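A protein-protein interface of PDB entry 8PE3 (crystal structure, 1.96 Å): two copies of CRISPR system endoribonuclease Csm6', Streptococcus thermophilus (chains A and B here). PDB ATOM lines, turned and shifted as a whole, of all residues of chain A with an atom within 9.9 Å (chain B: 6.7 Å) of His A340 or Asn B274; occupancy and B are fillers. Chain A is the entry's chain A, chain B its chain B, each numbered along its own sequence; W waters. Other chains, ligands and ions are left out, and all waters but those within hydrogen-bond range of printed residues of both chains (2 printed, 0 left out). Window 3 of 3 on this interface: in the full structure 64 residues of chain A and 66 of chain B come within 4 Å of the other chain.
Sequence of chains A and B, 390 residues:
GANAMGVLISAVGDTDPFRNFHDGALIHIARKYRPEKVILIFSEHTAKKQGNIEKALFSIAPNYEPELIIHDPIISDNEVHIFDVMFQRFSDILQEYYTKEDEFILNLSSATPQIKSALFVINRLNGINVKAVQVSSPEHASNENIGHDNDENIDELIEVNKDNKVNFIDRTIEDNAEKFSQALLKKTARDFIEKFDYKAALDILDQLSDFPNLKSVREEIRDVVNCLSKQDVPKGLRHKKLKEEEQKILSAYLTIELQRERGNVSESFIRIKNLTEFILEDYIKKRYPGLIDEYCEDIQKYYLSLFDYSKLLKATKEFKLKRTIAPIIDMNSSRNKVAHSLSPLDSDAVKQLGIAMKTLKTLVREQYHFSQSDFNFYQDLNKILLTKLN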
ATOM      1  N   SER A 266      25.036  14.101  20.508  1.00  0.00           N
ATOM      2  CA  SER A 266      23.595  14.319  20.626  1.00  0.00           C
ATOM      3  C   SER A 266      23.143  14.225  22.078  1.00  0.00           C
ATOM      4  O   SER A 266      22.269  14.982  22.517  1.00  0.00           O
ATOM      5  CB  SER A 266      22.819  13.329  19.752  1.00  0.00           C
ATOM      6  OG  SER A 266      23.417  12.047  19.742  1.00  0.00           O
ATOM      7  N   GLU A 267      23.739  13.319  22.850  1.00  0.00           N
ATOM      8  CA  GLU A 267      23.393  13.219  24.263  1.00  0.00           C
ATOM      9  C   GLU A 267      23.822  14.455  25.054  1.00  0.00           C
ATOM     10  O   GLU A 267      23.242  14.730  26.109  1.00  0.00           O
ATOM     11  CB  GLU A 267      24.016  11.953  24.857  1.00  0.00           C
ATOM     12  CG  GLU A 267      23.617  11.657  26.291  1.00  0.00           C
ATOM     13  CD  GLU A 267      24.586  10.711  26.972  1.00  0.00           C
ATOM     14  OE1 GLU A 267      25.065   9.769  26.297  1.00  0.00           O
ATOM     15  OE2 GLU A 267      24.875  10.912  28.175  1.00  0.00           O
ATOM     16  N   ILE A 270      20.823  17.318  25.735  1.00  0.00           N
ATOM     17  CA  ILE A 270      19.885  17.171  26.847  1.00  0.00           C
ATOM     18  C   ILE A 270      20.586  17.469  28.169  1.00  0.00           C
ATOM     19  O   ILE A 270      19.993  18.047  29.088  1.00  0.00           O
ATOM     20  CB  ILE A 270      19.247  15.769  26.835  1.00  0.00           C
ATOM     21  N   LYS A 273      21.089  21.335  28.795  1.00  0.00           N
ATOM     22  CA  LYS A 273      19.866  22.000  29.224  1.00  0.00           C
ATOM     23  C   LYS A 273      19.575  21.700  30.690  1.00  0.00           C
ATOM     24  O   LYS A 273      19.286  22.611  31.475  1.00  0.00           O
ATOM     25  CB  LYS A 273      18.698  21.583  28.332  1.00  0.00           C
ATOM     26  CG  LYS A 273      17.396  22.287  28.670  1.00  0.00           C
ATOM     27  CD  LYS A 273      16.271  21.864  27.738  1.00  0.00           C
ATOM     28  CE  LYS A 273      15.125  21.205  28.496  1.00  0.00           C
ATOM     29  NZ  LYS A 273      13.964  22.128  28.662  1.00  0.00           N
ATOM     30  N   ASN A 332      17.905  25.217  21.673  1.00  0.00           N
ATOM     31  CA  ASN A 332      16.724  24.537  22.192  1.00  0.00           C
ATOM     32  C   ASN A 332      16.074  23.675  21.118  1.00  0.00           C
ATOM     33  O   ASN A 332      15.563  22.590  21.415  1.00  0.00           O
ATOM     34  CB  ASN A 332      15.718  25.547  22.736  1.00  0.00           C
ATOM     35  CG  ASN A 332      14.471  24.880  23.285  1.00  0.00           C
ATOM     36  OD1 ASN A 332      14.542  24.100  24.242  1.00  0.00           O
ATOM     37  ND2 ASN A 332      13.323  25.164  22.669  1.00  0.00           N
ATOM     38  N   SER A 333      16.084  24.143  19.868  1.00  0.00           N
ATOM     39  CA  SER A 333      15.476  23.387  18.776  1.00  0.00           C
ATOM     40  C   SER A 333      16.201  22.064  18.554  1.00  0.00           C
ATOM     41  O   SER A 333      15.567  21.014  18.387  1.00  0.00           O
ATOM     42  CB  SER A 333      15.482  24.230  17.500  1.00  0.00           C
ATOM     43  OG  SER A 333      16.664  25.014  17.426  1.00  0.00           O
ATOM     44  N   SER A 334      17.538  22.096  18.556  1.00  0.00           N
ATOM     45  CA  SER A 334      18.324  20.877  18.377  1.00  0.00           C
ATOM     46  C   SER A 334      18.147  19.920  19.551  1.00  0.00           C
ATOM     47  O   SER A 334      18.025  18.704  19.353  1.00  0.00           O
ATOM     48  CB  SER A 334      19.799  21.229  18.195  1.00  0.00           C
ATOM     49  OG  SER A 334      20.032  21.749  16.901  1.00  0.00           O
ATOM     50  N   ARG A 335      18.146  20.451  20.782  1.00  0.00           N
ATOM     51  CA  ARG A 335      17.844  19.628  21.951  1.00  0.00           C
ATOM     52  C   ARG A 335      16.487  18.946  21.809  1.00  0.00           C
ATOM     53  O   ARG A 335      16.305  17.811  22.269  1.00  0.00           O
ATOM     54  CB  ARG A 335      17.906  20.480  23.229  1.00  0.00           C
ATOM     55  CG  ARG A 335      17.493  19.756  24.519  1.00  0.00           C
ATOM     56  CD  ARG A 335      15.980  19.876  24.764  1.00  0.00           C
ATOM     57  NE  ARG A 335      15.502  19.145  25.933  1.00  0.00           N
ATOM     58  CZ  ARG A 335      14.220  18.922  26.202  1.00  0.00           C
ATOM     59  NH1 ARG A 335      13.258  19.369  25.410  1.00  0.00           N
ATOM     60  NH2 ARG A 335      13.895  18.235  27.294  1.00  0.00           N
ATOM     61  N   ASN A 336      15.519  19.626  21.179  1.00  0.00           N
ATOM     62  CA  ASN A 336      14.199  19.035  20.957  1.00  0.00           C
ATOM     63  C   ASN A 336      14.258  17.865  19.977  1.00  0.00           C
ATOM     64  O   ASN A 336      13.478  16.912  20.106  1.00  0.00           O
ATOM     65  CB  ASN A 336      13.223  20.098  20.446  1.00  0.00           C
ATOM     66  CG  ASN A 336      12.687  20.987  21.558  1.00  0.00           C
ATOM     67  OD1 ASN A 336      12.781  20.646  22.740  1.00  0.00           O
ATOM     68  ND2 ASN A 336      12.127  22.138  21.182  1.00  0.00           N
ATOM     69  N   LYS A 337      15.170  17.916  18.999  1.00  0.00           N
ATOM     70  CA  LYS A 337      15.301  16.816  18.045  1.00  0.00           C
ATOM     71  C   LYS A 337      15.845  15.563  18.720  1.00  0.00           C
ATOM     72  O   LYS A 337      15.460  14.443  18.365  1.00  0.00           O
ATOM     73  N   VAL A 338      16.736  15.735  19.704  1.00  0.00           N
ATOM     74  CA  VAL A 338      17.311  14.602  20.427  1.00  0.00           C
ATOM     75  C   VAL A 338      16.429  14.136  21.576  1.00  0.00           C
ATOM     76  O   VAL A 338      16.694  13.080  22.165  1.00  0.00           O
ATOM     77  CB  VAL A 338      18.715  14.965  20.956  1.00  0.00           C
ATOM     78  CG1 VAL A 338      19.509  13.716  21.316  1.00  0.00           C
ATOM     79  CG2 VAL A 338      19.474  15.798  19.939  1.00  0.00           C
ATOM     80  N   ALA A 339      15.370  14.886  21.906  1.00  0.00           N
ATOM     81  CA  ALA A 339      14.537  14.573  23.060  1.00  0.00           C
ATOM     82  C   ALA A 339      13.135  14.090  22.718  1.00  0.00           C
ATOM     83  O   ALA A 339      12.513  13.434  23.560  1.00  0.00           O
ATOM     84  CB  ALA A 339      14.421  15.795  23.984  1.00  0.00           C
ATOM     85  N   HIS A 340      12.612  14.404  21.523  1.00  0.00           N
ATOM     86  CA  HIS A 340      11.280  13.953  21.130  1.00  0.00           C
ATOM     87  C   HIS A 340      11.246  13.496  19.674  1.00  0.00           C
ATOM     88  O   HIS A 340      10.183  13.513  19.042  1.00  0.00           O
ATOM     89  CB  HIS A 340      10.222  15.049  21.341  1.00  0.00           C
ATOM     90  CG  HIS A 340      10.420  15.868  22.582  1.00  0.00           C
ATOM     91  ND1 HIS A 340      10.133  15.393  23.845  1.00  0.00           N
ATOM     92  CD2 HIS A 340      10.861  17.139  22.750  1.00  0.00           C
ATOM     93  CE1 HIS A 340      10.397  16.332  24.738  1.00  0.00           C
ATOM     94  NE2 HIS A 340      10.839  17.401  24.099  1.00  0.00           N
ATOM     95  N   SER A 341      12.386  13.073  19.128  1.00  0.00           N
ATOM     96  CA  SER A 341      12.463  12.791  17.701  1.00  0.00           C
ATOM     97  C   SER A 341      13.627  11.847  17.423  1.00  0.00           C
ATOM     98  O   SER A 341      14.494  11.623  18.275  1.00  0.00           O
ATOM     99  CB  SER A 341      12.611  14.090  16.895  1.00  0.00           C
ATOM    100  OG  SER A 341      12.671  13.839  15.500  1.00  0.00           O
ATOM    101  N   LEU A 342      13.616  11.277  16.213  1.00  0.00           N
ATOM    102  CA  LEU A 342      14.752  10.552  15.659  1.00  0.00           C
ATOM    103  C   LEU A 342      15.347  11.279  14.464  1.00  0.00           C
ATOM    104  O   LEU A 342      16.053  10.670  13.653  1.00  0.00           O
ATOM    105  CB  LEU A 342      14.354   9.129  15.265  1.00  0.00           C
ATOM    106  CG  LEU A 342      13.982   8.206  16.421  1.00  0.00           C
ATOM    107  CD1 LEU A 342      13.906   6.758  15.966  1.00  0.00           C
ATOM    108  CD2 LEU A 342      14.981   8.361  17.550  1.00  0.00           C
ATOM    109  N   SER A 343      15.060  12.555  14.333  1.00  0.00           N
ATOM    110  CA  SER A 343      15.647  13.349  13.275  1.00  0.00           C
ATOM    111  C   SER A 343      17.091  13.694  13.637  1.00  0.00           C
ATOM    112  O   SER A 343      17.426  13.832  14.817  1.00  0.00           O
ATOM    113  CB  SER A 343      14.837  14.624  13.060  1.00  0.00           C
ATOM    114  OG  SER A 343      13.747  14.398  12.180  1.00  0.00           O
ATOM    115  N   PRO A 344      17.968  13.809  12.647  1.00  0.00           N
ATOM    116  CA  PRO A 344      19.387  14.019  12.930  1.00  0.00           C
ATOM    117  C   PRO A 344      19.764  15.492  12.981  1.00  0.00           C
ATOM    118  O   PRO A 344      19.068  16.363  12.459  1.00  0.00           O
ATOM    119  CB  PRO A 344      20.069  13.327  11.742  1.00  0.00           C
ATOM    120  CG  PRO A 344      19.114  13.562  10.617  1.00  0.00           C
ATOM    121  CD  PRO A 344      17.729  13.513  11.224  1.00  0.00           C
ATOM    122  N   LEU A 345      20.903  15.752  13.616  1.00  0.00           N
ATOM    123  CA  LEU A 345      21.437  17.100  13.725  1.00  0.00           C
ATOM    124  C   LEU A 345      22.308  17.427  12.520  1.00  0.00           C
ATOM    125  O   LEU A 345      22.976  16.556  11.960  1.00  0.00           O
ATOM    126  CB  LEU A 345      22.259  17.249  15.003  1.00  0.00           C
ATOM    127  CG  LEU A 345      21.574  16.780  16.281  1.00  0.00           C
ATOM    128  CD1 LEU A 345      22.509  16.965  17.465  1.00  0.00           C
ATOM    129  CD2 LEU A 345      20.259  17.520  16.481  1.00  0.00           C
ATOM    130  N   GLN B 231      23.195  11.796  15.508  1.00  0.00           N
ATOM    131  CA  GLN B 231      21.996  10.956  15.613  1.00  0.00           C
ATOM    132  C   GLN B 231      21.429  10.606  14.234  1.00  0.00           C
ATOM    133  O   GLN B 231      20.216  10.486  14.052  1.00  0.00           O
ATOM    134  CB  GLN B 231      20.935  11.610  16.507  1.00  0.00           C
ATOM    135  CG  GLN B 231      20.082  10.594  17.293  1.00  0.00           C
ATOM    136  CD  GLN B 231      18.825  11.192  17.942  1.00  0.00           C
ATOM    137  OE1 GLN B 231      18.332  12.249  17.536  1.00  0.00           O
ATOM    138  NE2 GLN B 231      18.304  10.503  18.956  1.00  0.00           N
ATOM    139  N   PHE B 269      17.532   6.149  29.040  1.00  0.00           N
ATOM    140  CA  PHE B 269      16.116   6.354  29.343  1.00  0.00           C
ATOM    141  C   PHE B 269      15.473   7.359  28.394  1.00  0.00           C
ATOM    142  O   PHE B 269      14.321   7.173  27.984  1.00  0.00           O
ATOM    143  CB  PHE B 269      15.921   6.767  30.806  1.00  0.00           C
ATOM    144  CG  PHE B 269      16.206   5.661  31.796  1.00  0.00           C
ATOM    145  CD1 PHE B 269      17.483   5.137  31.946  1.00  0.00           C
ATOM    146  CD2 PHE B 269      15.180   5.130  32.567  1.00  0.00           C
ATOM    147  CE1 PHE B 269      17.729   4.105  32.850  1.00  0.00           C
ATOM    148  CE2 PHE B 269      15.420   4.105  33.473  1.00  0.00           C
ATOM    149  CZ  PHE B 269      16.696   3.594  33.613  1.00  0.00           C
ATOM    150  N   ILE B 270      16.189   8.424  28.022  1.00  0.00           N
ATOM    151  CA  ILE B 270      15.604   9.369  27.072  1.00  0.00           C
ATOM    152  C   ILE B 270      15.594   8.771  25.670  1.00  0.00           C
ATOM    153  O   ILE B 270      14.691   9.047  24.870  1.00  0.00           O
ATOM    154  CB  ILE B 270      16.348  10.717  27.114  1.00  0.00           C
ATOM    155  N   ARG B 271      16.583   7.932  25.356  1.00  0.00           N
ATOM    156  CA  ARG B 271      16.626   7.285  24.051  1.00  0.00           C
ATOM    157  C   ARG B 271      15.472   6.303  23.894  1.00  0.00           C
ATOM    158  O   ARG B 271      14.864   6.217  22.820  1.00  0.00           O
ATOM    159  CB  ARG B 271      17.967   6.570  23.885  1.00  0.00           C
ATOM    160  CG  ARG B 271      19.126   7.458  23.424  1.00  0.00           C
ATOM    161  CD  ARG B 271      20.328   6.609  22.984  1.00  0.00           C
ATOM    162  NE  ARG B 271      21.583   7.357  22.976  1.00  0.00           N
ATOM    163  CZ  ARG B 271      21.970   8.191  22.018  1.00  0.00           C
ATOM    164  NH1 ARG B 271      21.231   8.397  20.935  1.00  0.00           N
ATOM    165  NH2 ARG B 271      23.131   8.834  22.150  1.00  0.00           N
ATOM    166  N   ILE B 272      15.154   5.563  24.961  1.00  0.00           N
ATOM    167  CA  ILE B 272      14.090   4.566  24.897  1.00  0.00           C
ATOM    168  C   ILE B 272      12.736   5.240  24.732  1.00  0.00           C
ATOM    169  O   ILE B 272      11.850   4.723  24.038  1.00  0.00           O
ATOM    170  CB  ILE B 272      14.126   3.666  26.146  1.00  0.00           C
ATOM    171  CG1 ILE B 272      15.184   2.580  25.985  1.00  0.00           C
ATOM    172  CG2 ILE B 272      12.761   3.037  26.407  1.00  0.00           C
ATOM    173  CD1 ILE B 272      15.782   2.124  27.295  1.00  0.00           C
ATOM    174  N   LYS B 273      12.552   6.405  25.358  1.00  0.00           N
ATOM    175  CA  LYS B 273      11.282   7.108  25.234  1.00  0.00           C
ATOM    176  C   LYS B 273      11.054   7.561  23.797  1.00  0.00           C
ATOM    177  O   LYS B 273       9.993   7.308  23.217  1.00  0.00           O
ATOM    178  CB  LYS B 273      11.234   8.298  26.197  1.00  0.00           C
ATOM    179  CG  LYS B 273       9.829   8.844  26.419  1.00  0.00           C
ATOM    180  CD  LYS B 273       9.825  10.281  26.924  1.00  0.00           C
ATOM    181  N   ASN B 274      12.057   8.207  23.193  1.00  0.00           N
ATOM    182  CA  ASN B 274      11.900   8.687  21.822  1.00  0.00           C
ATOM    183  C   ASN B 274      11.720   7.537  20.847  1.00  0.00           C
ATOM    184  O   ASN B 274      10.884   7.610  19.941  1.00  0.00           O
ATOM    185  CB  ASN B 274      13.092   9.541  21.413  1.00  0.00           C
ATOM    186  CG  ASN B 274      13.348  10.667  22.374  1.00  0.00           C
ATOM    187  OD1 ASN B 274      14.466  11.170  22.474  1.00  0.00           O
ATOM    188  ND2 ASN B 274      12.303  11.087  23.082  1.00  0.00           N
ATOM    189  N   LEU B 275      12.498   6.466  21.009  1.00  0.00           N
ATOM    190  CA  LEU B 275      12.340   5.333  20.111  1.00  0.00           C
ATOM    191  C   LEU B 275      10.957   4.715  20.261  1.00  0.00           C
ATOM    192  O   LEU B 275      10.319   4.360  19.263  1.00  0.00           O
ATOM    193  CB  LEU B 275      13.437   4.299  20.357  1.00  0.00           C
ATOM    194  CG  LEU B 275      13.314   3.059  19.472  1.00  0.00           C
ATOM    195  CD1 LEU B 275      13.316   3.469  18.005  1.00  0.00           C
ATOM    196  CD2 LEU B 275      14.432   2.070  19.759  1.00  0.00           C
ATOM    197  N   THR B 276      10.460   4.605  21.495  1.00  0.00           N
ATOM    198  CA  THR B 276       9.115   4.074  21.689  1.00  0.00           C
ATOM    199  C   THR B 276       8.068   5.027  21.126  1.00  0.00           C
ATOM    200  O   THR B 276       7.124   4.599  20.452  1.00  0.00           O
ATOM    201  CB  THR B 276       8.862   3.806  23.172  1.00  0.00           C
ATOM    202  OG1 THR B 276       9.683   2.712  23.605  1.00  0.00           O
ATOM    203  CG2 THR B 276       7.411   3.434  23.400  1.00  0.00           C
ATOM    204  N   GLU B 277       8.232   6.327  21.378  1.00  0.00           N
ATOM    205  CA  GLU B 277       7.326   7.312  20.802  1.00  0.00           C
ATOM    206  C   GLU B 277       7.336   7.242  19.280  1.00  0.00           C
ATOM    207  O   GLU B 277       6.283   7.357  18.640  1.00  0.00           O
ATOM    208  CB  GLU B 277       7.704   8.717  21.277  1.00  0.00           C
ATOM    209  CG  GLU B 277       7.357   8.995  22.735  1.00  0.00           C
ATOM    210  CD  GLU B 277       7.837  10.357  23.232  1.00  0.00           C
ATOM    211  OE1 GLU B 277       8.610  11.036  22.515  1.00  0.00           O
ATOM    212  OE2 GLU B 277       7.427  10.744  24.350  1.00  0.00           O
ATOM    213  N   PHE B 278       8.516   7.040  18.684  1.00  0.00           N
ATOM    214  CA  PHE B 278       8.624   7.002  17.227  1.00  0.00           C
ATOM    215  C   PHE B 278       7.983   5.743  16.661  1.00  0.00           C
ATOM    216  O   PHE B 278       7.367   5.778  15.589  1.00  0.00           O
ATOM    217  CB  PHE B 278      10.095   7.092  16.816  1.00  0.00           C
ATOM    218  CG  PHE B 278      10.319   7.162  15.326  1.00  0.00           C
ATOM    219  CD1 PHE B 278      10.393   6.008  14.564  1.00  0.00           C
ATOM    220  CD2 PHE B 278      10.484   8.387  14.696  1.00  0.00           C
ATOM    221  CE1 PHE B 278      10.605   6.078  13.202  1.00  0.00           C
ATOM    222  CE2 PHE B 278      10.703   8.460  13.332  1.00  0.00           C
ATOM    223  CZ  PHE B 278      10.762   7.307  12.587  1.00  0.00           C
ATOM    224  N   ILE B 279       8.118   4.622  17.368  1.00  0.00           N
ATOM    225  CA  ILE B 279       7.501   3.378  16.921  1.00  0.00           C
ATOM    226  C   ILE B 279       5.980   3.490  16.964  1.00  0.00           C
ATOM    227  O   ILE B 279       5.283   3.117  16.013  1.00  0.00           O
ATOM    228  CB  ILE B 279       8.009   2.206  17.774  1.00  0.00           C
ATOM    229  CG1 ILE B 279       9.489   1.966  17.481  1.00  0.00           C
ATOM    230  CG2 ILE B 279       7.174   0.957  17.528  1.00  0.00           C
ATOM    231  CD1 ILE B 279      10.168   1.090  18.483  1.00  0.00           C
ATOM    232  N   GLU B 281       4.063   6.183  16.912  1.00  0.00           N
ATOM    233  CA  GLU B 281       3.537   7.089  15.898  1.00  0.00           C
ATOM    234  C   GLU B 281       3.612   6.454  14.515  1.00  0.00           C
ATOM    235  O   GLU B 281       2.701   6.620  13.696  1.00  0.00           O
ATOM    236  CB  GLU B 281       4.290   8.415  15.920  1.00  0.00           C
ATOM    237  CG  GLU B 281       4.142   9.214  14.637  1.00  0.00           C
ATOM    238  CD  GLU B 281       4.981  10.477  14.627  1.00  0.00           C
ATOM    239  OE1 GLU B 281       4.434  11.541  14.257  1.00  0.00           O
ATOM    240  OE2 GLU B 281       6.189  10.399  14.958  1.00  0.00           O
ATOM    241  N   TYR B 303       4.758  18.713  19.967  1.00  0.00           N
ATOM    242  CA  TYR B 303       5.189  17.314  19.898  1.00  0.00           C
ATOM    243  C   TYR B 303       4.389  16.398  20.839  1.00  0.00           C
ATOM    244  O   TYR B 303       4.178  16.726  22.004  1.00  0.00           O
ATOM    245  N   LEU B 304       3.954  15.246  20.327  1.00  0.00           N
ATOM    246  CA  LEU B 304       3.145  14.313  21.103  1.00  0.00           C
ATOM    247  C   LEU B 304       4.023  13.430  21.979  1.00  0.00           C
ATOM    248  O   LEU B 304       5.171  13.130  21.644  1.00  0.00           O
ATOM    249  CB  LEU B 304       2.305  13.431  20.181  1.00  0.00           C
ATOM    250  CG  LEU B 304       0.792  13.649  20.177  1.00  0.00           C
ATOM    251  CD1 LEU B 304       0.463  15.098  19.858  1.00  0.00           C
ATOM    252  CD2 LEU B 304       0.125  12.705  19.175  1.00  0.00           C
ATOM    253  N   SER B 305       3.463  12.986  23.096  1.00  0.00           N
ATOM    254  CA  SER B 305       4.226  12.261  24.099  1.00  0.00           C
ATOM    255  C   SER B 305       3.661  10.861  24.300  1.00  0.00           C
ATOM    256  O   SER B 305       2.594  10.508  23.789  1.00  0.00           O
ATOM    257  CB  SER B 305       4.234  13.021  25.429  1.00  0.00           C
ATOM    258  OG  SER B 305       3.262  12.497  26.317  1.00  0.00           O
ATOM    259  N   LEU B 306       4.410  10.064  25.071  1.00  0.00           N
ATOM    260  CA  LEU B 306       3.996   8.703  25.397  1.00  0.00           C
ATOM    261  C   LEU B 306       2.592   8.660  25.977  1.00  0.00           C
ATOM    262  O   LEU B 306       1.845   7.699  25.742  1.00  0.00           O
ATOM    263  CB  LEU B 306       4.986   8.086  26.383  1.00  0.00           C
ATOM    264  CG  LEU B 306       5.494   6.671  26.125  1.00  0.00           C
ATOM    265  CD1 LEU B 306       5.912   6.501  24.682  1.00  0.00           C
ATOM    266  CD2 LEU B 306       6.658   6.371  27.056  1.00  0.00           C
ATOM    267  N   ARG B 335      13.233   8.614  34.203  1.00  0.00           N
ATOM    268  CA  ARG B 335      13.714   9.373  33.050  1.00  0.00           C
ATOM    269  C   ARG B 335      13.635  10.882  33.277  1.00  0.00           C
ATOM    270  O   ARG B 335      14.284  11.644  32.550  1.00  0.00           O
ATOM    271  CB  ARG B 335      12.918   8.944  31.803  1.00  0.00           C
ATOM    272  CG  ARG B 335      13.174   9.708  30.499  1.00  0.00           C
ATOM    273  CD  ARG B 335      11.979  10.593  30.136  1.00  0.00           C
ATOM    274  NE  ARG B 335      12.283  11.593  29.116  1.00  0.00           N
ATOM    275  CZ  ARG B 335      11.600  12.717  28.938  1.00  0.00           C
ATOM    276  NH1 ARG B 335      10.593  13.047  29.732  1.00  0.00           N
ATOM    277  NH2 ARG B 335      11.931  13.528  27.934  1.00  0.00           N
HETATM  278  O   HOH W   1      10.240  10.228  19.022  1.00  0.00           O
HETATM  279  O   HOH W   2      18.113   8.665  13.110  1.00  0.00           O
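The backbone carbonyl oxygen of Val A338 lies close to the side-chain amide oxygen of Asn B274. OE1 of Gln B231 sits close to O of Ser A343, 3.3 Å away. O of Ala A339 sits at hydrogen-bond distance from ND2 of Asn B274 (2.4 Å).
The guanidinium group (NH1) of Arg A335 lies within hydrogen-bond range of a ring nitrogen (NE2) of His A340. OG of Ser A341 sits at hydrogen-bond distance from N of Ser A343, 3.0 Å away. OD1 of Asn B274 lies close to O of Ile B270.
Lys A337 touches Gln B231. Val A338 touches Gln B231. ND2 of Asn B274 touches CA of His A340 (3.6 Å). OE1 of Gln B231 touches O of Ser A341, at 3.96 Å. Leu B275 touches Leu A342. CD1 of Leu A342 touches CG of Phe B278, at 3.7 Å. CB of Pro A344 touches O of Gln B231 (3.7 Å).
Glu A267 touches none of the printed residues of chain B. Of the printed residues of chain B, Val A338 touches Gln B231 (3.9 Å) and Asn B274 (3.0 Å). Of the printed residues of chain B, Ser A341 touches Gln B231. No residue of chain A comes within 4 Å of Lys B273. Of the printed residues of chain A, Asn B274 touches Val A338, Ala A339 and His A340. No residue of chain A comes within 4 Å of Glu B277. Arg B335 touches none of the printed residues of chain A. The nearest residue of chain B that does not touch His A340 is Glu B277 (4.2 Å).
Printed residues of chain A that touch a printed residue of chain B: Lys A337, Val A338, Ala A339, His A340, Ser A341, Leu A342, Ser A343 and Pro A344. Of the 18 printed residues of chain B, 4 touch a printed residue of chain A. Printed residues of chain B that touch a printed residue of chain A: Gln B231, Asn B274, Leu B275 and Phe B278. Hydrophobic or aromatic side chains of chain B that line the printed part of chain A: Leu B275 and Phe B278. Among the printed residues, 10 pairs touch across the chains.
3 positions are printed for both chains.
Water W1 bridges the backbone carbonyl oxygen of Asn B274 and the backbone carbonyl oxygen of His A340. Water W2 bridges the backbone carbonyl oxygen (O) of Leu A342 and the backbone carbonyl oxygen (O) of Gln B231.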
